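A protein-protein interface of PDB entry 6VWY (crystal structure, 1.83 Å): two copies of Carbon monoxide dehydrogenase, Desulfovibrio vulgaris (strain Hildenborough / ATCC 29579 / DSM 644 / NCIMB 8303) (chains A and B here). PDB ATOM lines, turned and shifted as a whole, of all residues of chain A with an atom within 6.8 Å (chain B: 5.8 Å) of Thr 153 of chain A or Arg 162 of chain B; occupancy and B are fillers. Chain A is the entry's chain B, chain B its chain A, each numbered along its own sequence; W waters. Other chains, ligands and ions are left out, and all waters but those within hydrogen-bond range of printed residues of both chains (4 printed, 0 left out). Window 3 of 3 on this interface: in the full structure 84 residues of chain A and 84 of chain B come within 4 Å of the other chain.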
ATOM      1  N   ILE A 105      22.389 -19.128  23.110  1.00  0.00           N
ATOM      2  CA  ILE A 105      21.417 -20.214  23.062  1.00  0.00           C
ATOM      3  C   ILE A 105      20.978 -20.459  21.629  1.00  0.00           C
ATOM      4  O   ILE A 105      20.865 -21.611  21.189  1.00  0.00           O
ATOM      5  CB  ILE A 105      20.198 -19.922  23.952  1.00  0.00           C
ATOM      6  CG1 ILE A 105      20.611 -19.548  25.378  1.00  0.00           C
ATOM      7  CG2 ILE A 105      19.303 -21.152  23.986  1.00  0.00           C
ATOM      8  CD1 ILE A 105      19.447 -18.973  26.162  1.00  0.00           C
ATOM      9  N   GLU A 109      21.421 -23.923  19.539  1.00  0.00           N
ATOM     10  CA  GLU A 109      20.260 -24.551  18.923  1.00  0.00           C
ATOM     11  C   GLU A 109      20.467 -24.742  17.422  1.00  0.00           C
ATOM     12  O   GLU A 109      20.116 -25.789  16.868  1.00  0.00           O
ATOM     13  CB  GLU A 109      19.009 -23.714  19.192  1.00  0.00           C
ATOM     14  CG  GLU A 109      17.780 -24.239  18.489  1.00  0.00           C
ATOM     15  CD  GLU A 109      16.551 -23.385  18.752  1.00  0.00           C
ATOM     16  OE1 GLU A 109      15.487 -23.961  19.042  1.00  0.00           O
ATOM     17  OE2 GLU A 109      16.656 -22.145  18.680  1.00  0.00           O
ATOM     18  N   GLU A 113      20.448 -28.353  15.484  1.00  0.00           N
ATOM     19  CA  GLU A 113      19.600 -28.602  14.321  1.00  0.00           C
ATOM     20  C   GLU A 113      20.384 -28.875  13.045  1.00  0.00           C
ATOM     21  O   GLU A 113      19.762 -29.172  12.020  1.00  0.00           O
ATOM     22  CB  GLU A 113      18.683 -27.399  14.066  1.00  0.00           C
ATOM     23  CG  GLU A 113      17.656 -27.127  15.152  1.00  0.00           C
ATOM     24  CD  GLU A 113      16.945 -25.784  14.962  1.00  0.00           C
ATOM     25  OE1 GLU A 113      17.458 -24.923  14.207  1.00  0.00           O
ATOM     26  OE2 GLU A 113      15.873 -25.588  15.571  1.00  0.00           O
ATOM     27  N   ALA A 148      22.281 -31.400  23.346  1.00  0.00           N
ATOM     28  CA  ALA A 148      22.337 -29.957  23.127  1.00  0.00           C
ATOM     29  C   ALA A 148      20.943 -29.355  22.986  1.00  0.00           C
ATOM     30  O   ALA A 148      20.678 -28.264  23.506  1.00  0.00           O
ATOM     31  CB  ALA A 148      23.173 -29.645  21.885  1.00  0.00           C
ATOM     32  N   ALA A 149      20.034 -30.047  22.294  1.00  0.00           N
ATOM     33  CA  ALA A 149      18.674 -29.522  22.160  1.00  0.00           C
ATOM     34  C   ALA A 149      17.965 -29.432  23.514  1.00  0.00           C
ATOM     35  O   ALA A 149      17.165 -28.511  23.741  1.00  0.00           O
ATOM     36  CB  ALA A 149      17.870 -30.397  21.194  1.00  0.00           C
ATOM     37  N   ASP A 150      18.256 -30.356  24.431  1.00  0.00           N
ATOM     38  CA  ASP A 150      17.595 -30.343  25.738  1.00  0.00           C
ATOM     39  C   ASP A 150      18.190 -29.275  26.642  1.00  0.00           C
ATOM     40  O   ASP A 150      17.460 -28.637  27.410  1.00  0.00           O
ATOM     41  CB  ASP A 150      17.687 -31.720  26.406  1.00  0.00           C
ATOM     42  CG  ASP A 150      16.651 -32.686  25.874  1.00  0.00           C
ATOM     43  OD1 ASP A 150      15.786 -32.244  25.100  1.00  0.00           O
ATOM     44  OD2 ASP A 150      16.690 -33.878  26.223  1.00  0.00           O
ATOM     45  N   LEU A 151      19.508 -29.061  26.549  1.00  0.00           N
ATOM     46  CA  LEU A 151      20.130 -27.938  27.245  1.00  0.00           C
ATOM     47  C   LEU A 151      19.605 -26.610  26.711  1.00  0.00           C
ATOM     48  O   LEU A 151      19.350 -25.679  27.486  1.00  0.00           O
ATOM     49  CB  LEU A 151      21.659 -28.006  27.119  1.00  0.00           C
ATOM     50  CG  LEU A 151      22.460 -26.852  27.746  1.00  0.00           C
ATOM     51  CD1 LEU A 151      22.161 -26.726  29.247  1.00  0.00           C
ATOM     52  CD2 LEU A 151      23.958 -27.091  27.567  1.00  0.00           C
ATOM     53  N   VAL A 152      19.438 -26.502  25.390  1.00  0.00           N
ATOM     54  CA  VAL A 152      18.858 -25.292  24.808  1.00  0.00           C
ATOM     55  C   VAL A 152      17.487 -25.016  25.418  1.00  0.00           C
ATOM     56  O   VAL A 152      17.178 -23.881  25.799  1.00  0.00           O
ATOM     57  CB  VAL A 152      18.799 -25.423  23.271  1.00  0.00           C
ATOM     58  CG1 VAL A 152      17.778 -24.459  22.677  1.00  0.00           C
ATOM     59  CG2 VAL A 152      20.181 -25.188  22.671  1.00  0.00           C
ATOM     60  N   THR A 153      16.662 -26.053  25.555  1.00  0.00           N
ATOM     61  CA  THR A 153      15.336 -25.884  26.146  1.00  0.00           C
ATOM     62  C   THR A 153      15.420 -25.392  27.589  1.00  0.00           C
ATOM     63  O   THR A 153      14.657 -24.506  27.994  1.00  0.00           O
ATOM     64  CB  THR A 153      14.575 -27.206  26.063  1.00  0.00           C
ATOM     65  OG1 THR A 153      14.296 -27.492  24.686  1.00  0.00           O
ATOM     66  CG2 THR A 153      13.267 -27.146  26.857  1.00  0.00           C
ATOM     67  N   ILE A 154      16.347 -25.942  28.374  1.00  0.00           N
ATOM     68  CA  ILE A 154      16.529 -25.488  29.754  1.00  0.00           C
ATOM     69  C   ILE A 154      16.939 -24.021  29.783  1.00  0.00           C
ATOM     70  O   ILE A 154      16.401 -23.224  30.561  1.00  0.00           O
ATOM     71  CB  ILE A 154      17.562 -26.364  30.484  1.00  0.00           C
ATOM     72  CG1 ILE A 154      17.027 -27.786  30.686  1.00  0.00           C
ATOM     73  CG2 ILE A 154      17.950 -25.718  31.812  1.00  0.00           C
ATOM     74  CD1 ILE A 154      18.054 -28.760  31.324  1.00  0.00           C
ATOM     75  N   CYS A 155      17.895 -23.638  28.929  1.00  0.00           N
ATOM     76  CA  CYS A 155      18.340 -22.243  28.924  1.00  0.00           C
ATOM     77  C   CYS A 155      17.230 -21.307  28.460  1.00  0.00           C
ATOM     78  O   CYS A 155      17.061 -20.218  29.012  1.00  0.00           O
ATOM     79  CB  CYS A 155      19.568 -22.075  28.038  1.00  0.00           C
ATOM     80  SG  CYS A 155      20.987 -22.966  28.693  1.00  0.00           S
ATOM     81  N   TYR A 156      16.482 -21.701  27.430  1.00  0.00           N
ATOM     82  CA  TYR A 156      15.372 -20.865  26.987  1.00  0.00           C
ATOM     83  C   TYR A 156      14.325 -20.721  28.083  1.00  0.00           C
ATOM     84  O   TYR A 156      13.712 -19.656  28.231  1.00  0.00           O
ATOM     85  CB  TYR A 156      14.744 -21.460  25.733  1.00  0.00           C
ATOM     86  CG  TYR A 156      15.299 -20.938  24.433  1.00  0.00           C
ATOM     87  CD1 TYR A 156      15.523 -19.578  24.244  1.00  0.00           C
ATOM     88  CD2 TYR A 156      15.589 -21.807  23.381  1.00  0.00           C
ATOM     89  CE1 TYR A 156      16.017 -19.093  23.044  1.00  0.00           C
ATOM     90  CE2 TYR A 156      16.074 -21.329  22.182  1.00  0.00           C
ATOM     91  CZ  TYR A 156      16.285 -19.975  22.020  1.00  0.00           C
ATOM     92  OH  TYR A 156      16.785 -19.499  20.824  1.00  0.00           O
ATOM     93  N   ASN A 157      14.087 -21.787  28.855  1.00  0.00           N
ATOM     94  CA  ASN A 157      13.092 -21.670  29.922  1.00  0.00           C
ATOM     95  C   ASN A 157      13.526 -20.676  30.992  1.00  0.00           C
ATOM     96  O   ASN A 157      12.680 -20.064  31.645  1.00  0.00           O
ATOM     97  CB  ASN A 157      12.799 -23.034  30.547  1.00  0.00           C
ATOM     98  CG  ASN A 157      12.038 -23.960  29.608  1.00  0.00           C
ATOM     99  OD1 ASN A 157      11.393 -23.514  28.668  1.00  0.00           O
ATOM    100  ND2 ASN A 157      12.116 -25.258  29.863  1.00  0.00           N
ATOM    101  N   ASP A 158      14.828 -20.477  31.179  1.00  0.00           N
ATOM    102  CA  ASP A 158      15.256 -19.403  32.068  1.00  0.00           C
ATOM    103  C   ASP A 158      14.982 -18.021  31.473  1.00  0.00           C
ATOM    104  O   ASP A 158      14.977 -17.024  32.209  1.00  0.00           O
ATOM    105  CB  ASP A 158      16.733 -19.570  32.406  1.00  0.00           C
ATOM    106  CG  ASP A 158      16.954 -20.470  33.624  1.00  0.00           C
ATOM    107  OD1 ASP A 158      16.003 -21.158  34.056  1.00  0.00           O
ATOM    108  OD2 ASP A 158      18.079 -20.473  34.157  1.00  0.00           O
ATOM    109  N   PHE A 159      14.733 -17.939  30.167  1.00  0.00           N
ATOM    110  CA  PHE A 159      14.283 -16.708  29.535  1.00  0.00           C
ATOM    111  C   PHE A 159      12.772 -16.677  29.397  1.00  0.00           C
ATOM    112  O   PHE A 159      12.238 -15.889  28.606  1.00  0.00           O
ATOM    113  CB  PHE A 159      14.954 -16.541  28.168  1.00  0.00           C
ATOM    114  CG  PHE A 159      16.372 -16.045  28.246  1.00  0.00           C
ATOM    115  CD1 PHE A 159      17.419 -16.914  28.501  1.00  0.00           C
ATOM    116  CD2 PHE A 159      16.654 -14.702  28.060  1.00  0.00           C
ATOM    117  CE1 PHE A 159      18.720 -16.457  28.562  1.00  0.00           C
ATOM    118  CE2 PHE A 159      17.963 -14.239  28.104  1.00  0.00           C
ATOM    119  CZ  PHE A 159      18.989 -15.107  28.365  1.00  0.00           C
ATOM    120  N   ASN B 157       4.043 -18.888  26.905  1.00  0.00           N
ATOM    121  CA  ASN B 157       5.008 -19.019  25.812  1.00  0.00           C
ATOM    122  C   ASN B 157       5.223 -17.695  25.078  1.00  0.00           C
ATOM    123  O   ASN B 157       6.310 -17.457  24.537  1.00  0.00           O
ATOM    124  CB  ASN B 157       4.565 -20.111  24.845  1.00  0.00           C
ATOM    125  CG  ASN B 157       4.809 -21.499  25.402  1.00  0.00           C
ATOM    126  OD1 ASN B 157       5.572 -21.659  26.350  1.00  0.00           O
ATOM    127  ND2 ASN B 157       4.169 -22.501  24.818  1.00  0.00           N
ATOM    128  N   GLY B 160       8.000 -15.999  26.645  1.00  0.00           N
ATOM    129  CA  GLY B 160       9.256 -16.682  26.473  1.00  0.00           C
ATOM    130  C   GLY B 160       9.984 -16.188  25.238  1.00  0.00           C
ATOM    131  O   GLY B 160       9.618 -15.186  24.619  1.00  0.00           O
ATOM    132  N   SER B 161      11.034 -16.922  24.883  1.00  0.00           N
ATOM    133  CA  SER B 161      12.002 -16.447  23.902  1.00  0.00           C
ATOM    134  C   SER B 161      12.095 -17.354  22.678  1.00  0.00           C
ATOM    135  O   SER B 161      13.096 -17.309  21.954  1.00  0.00           O
ATOM    136  CB  SER B 161      13.381 -16.306  24.557  1.00  0.00           C
ATOM    137  OG  SER B 161      14.296 -15.654  23.686  1.00  0.00           O
ATOM    138  N   ARG B 162      11.077 -18.173  22.416  1.00  0.00           N
ATOM    139  CA  ARG B 162      11.170 -19.142  21.334  1.00  0.00           C
ATOM    140  C   ARG B 162      10.158 -18.944  20.214  1.00  0.00           C
ATOM    141  O   ARG B 162      10.158 -19.735  19.268  1.00  0.00           O
ATOM    142  CB  ARG B 162      11.033 -20.573  21.886  1.00  0.00           C
ATOM    143  CG  ARG B 162      12.073 -20.911  22.947  1.00  0.00           C
ATOM    144  CD  ARG B 162      12.112 -22.436  23.254  1.00  0.00           C
ATOM    145  NE  ARG B 162      12.849 -23.176  22.236  1.00  0.00           N
ATOM    146  CZ  ARG B 162      13.334 -24.404  22.410  1.00  0.00           C
ATOM    147  NH1 ARG B 162      13.139 -25.030  23.559  1.00  0.00           N
ATOM    148  NH2 ARG B 162      14.025 -25.002  21.444  1.00  0.00           N
ATOM    149  N   ARG B 163       9.300 -17.931  20.297  1.00  0.00           N
ATOM    150  CA  ARG B 163       8.314 -17.683  19.257  1.00  0.00           C
ATOM    151  C   ARG B 163       8.915 -16.851  18.134  1.00  0.00           C
ATOM    152  O   ARG B 163       9.854 -16.078  18.340  1.00  0.00           O
ATOM    153  CB  ARG B 163       7.100 -16.938  19.816  1.00  0.00           C
ATOM    154  CG  ARG B 163       6.526 -17.467  21.125  1.00  0.00           C
ATOM    155  CD  ARG B 163       5.310 -18.326  20.865  1.00  0.00           C
ATOM    156  NE  ARG B 163       4.286 -17.597  20.117  1.00  0.00           N
ATOM    157  CZ  ARG B 163       3.411 -18.178  19.305  1.00  0.00           C
ATOM    158  NH1 ARG B 163       3.436 -19.494  19.131  1.00  0.00           N
ATOM    159  NH2 ARG B 163       2.520 -17.448  18.661  1.00  0.00           N
ATOM    160  N   ASN B 164       8.349 -17.003  16.933  1.00  0.00           N
ATOM    161  CA  ASN B 164       8.621 -16.077  15.839  1.00  0.00           C
ATOM    162  C   ASN B 164       7.590 -14.962  15.752  1.00  0.00           C
ATOM    163  O   ASN B 164       7.852 -13.932  15.115  1.00  0.00           O
ATOM    164  CB  ASN B 164       8.654 -16.820  14.507  1.00  0.00           C
ATOM    165  CG  ASN B 164       9.864 -17.712  14.386  1.00  0.00           C
ATOM    166  OD1 ASN B 164       9.748 -18.898  14.094  1.00  0.00           O
ATOM    167  ND2 ASN B 164      11.031 -17.148  14.633  1.00  0.00           N
ATOM    168  N   ARG B 192      10.803 -10.280  25.837  1.00  0.00           N
ATOM    169  CA  ARG B 192      11.996 -10.220  25.004  1.00  0.00           C
ATOM    170  C   ARG B 192      12.172  -8.845  24.365  1.00  0.00           C
ATOM    171  O   ARG B 192      13.286  -8.307  24.338  1.00  0.00           O
ATOM    172  CB  ARG B 192      11.947 -11.292  23.923  1.00  0.00           C
ATOM    173  CG  ARG B 192      13.192 -11.240  23.067  1.00  0.00           C
ATOM    174  CD  ARG B 192      13.167 -12.235  21.945  1.00  0.00           C
ATOM    175  NE  ARG B 192      14.450 -12.205  21.259  1.00  0.00           N
ATOM    176  CZ  ARG B 192      14.780 -12.996  20.249  1.00  0.00           C
ATOM    177  NH1 ARG B 192      13.903 -13.888  19.801  1.00  0.00           N
ATOM    178  NH2 ARG B 192      15.990 -12.890  19.696  1.00  0.00           N
HETATM  179  O   HOH W   1      13.447 -22.194  19.616  1.00  0.00           O
HETATM  180  O   HOH W   2      10.812 -24.560  25.530  1.00  0.00           O
HETATM  181  O   HOH W   3      15.382 -27.524  21.792  1.00  0.00           O
HETATM  182  O   HOH W   4      11.782 -19.064  26.356  1.00  0.00           O
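OE2 of Glu 109 of chain A lies within hydrogen-bond range of OH of Tyr 156 of chain A (3.4 Å).
The backbone carbonyl oxygen of Ala 149 of chain A is in hydrogen-bond range of the side-chain hydroxyl of Thr 153 of chain A (3.2 Å).
ND2 of Asn 157 of chain A lies close to O of Thr 153 of chain A.
Water W4 lies within hydrogen-bond range of N of Ser 161 of chain B and O of Tyr 156 of chain A.
Water W1 bridges the side-chain carboxylate (OE1) of Glu 109 of chain A (2.8 Å) and the guanidinium group (NE) of Arg 162 of chain B (2.9 Å).
Water W3 lies within hydrogen-bond range of the backbone carbonyl oxygen of Ala 149 of chain A (2.8 Å), the guanidinium group of Arg 162 of chain B (2.9 Å) and the side-chain hydroxyl of Thr 153 of chain A (3.1 Å).
Water W2 lies within hydrogen-bond range of NH1 of Arg 162 of chain B (3.1 Å) and OD1 of Asn 157 of chain A (3.4 Å).
The guanidinium group (NH2) of Arg 162 of chain B lies within salt-bridge range of the side-chain carboxylate (OE1) of Glu 109 of chain A (3.0 Å).
The side-chain hydroxyl (OG1) of Thr 153 of chain A lies within hydrogen-bond range of the guanidinium group (NH1) of Arg 162 of chain B.
Among the printed residues, merely in contact across the chains: Val 152 of chain A with Arg 162 of chain B (3.99 Å), Tyr 156 of chain A with Ser 161 of chain B (3.6 Å), Tyr 156 of chain A with Arg 162 of chain B (3.3 Å), Phe 159 of chain A with Gly 160 of chain B (3.8 Å) and Phe 159 of chain A with Ser 161 of chain B (3.9 Å).
Printed residues of chain B that touch a printed residue of chain A: Gly 160, Ser 161 and Arg 162.
Hydrophobic or aromatic side chains of chain A that line the printed part of chain B: Val 152, Tyr 156 and Phe 159.
Among the printed residues, Asp or Glu carboxylates within 4 Å of a Lys or Arg side-chain nitrogen of the other chain: Glu 109 of chain A with Arg 162 of chain B (3.0 Å).
Thr 153 of chain A touches just one residue of chain B: Arg 162 (2.9 Å).
Printed residues of chain A within 4 Å of Arg 162 of chain B: Glu 109, Val 152, Thr 153 and Tyr 156.
Of the printed residues of chain B, Phe 159 of chain A touches Gly 160 and Ser 161.
Of the printed residues of chain B, Glu 109 of chain A touches Arg 162 (3.0 Å).
Of the printed residues of chain B, Val 152 of chain A touches Arg 162.
Printed residues of chain A within 4 Å of Ser 161 of chain B: Tyr 156 (3.6 Å) and Phe 159 (3.9 Å).
Asn 164 of chain B touches none of the printed residues of chain A.
Arg 192 of chain B touches none of the printed residues of chain A.
Position printed for both chains: 157.
Of the 7 pairs that touch across the chains among the printed residues, none has its exchanged pair printed and touching as well.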
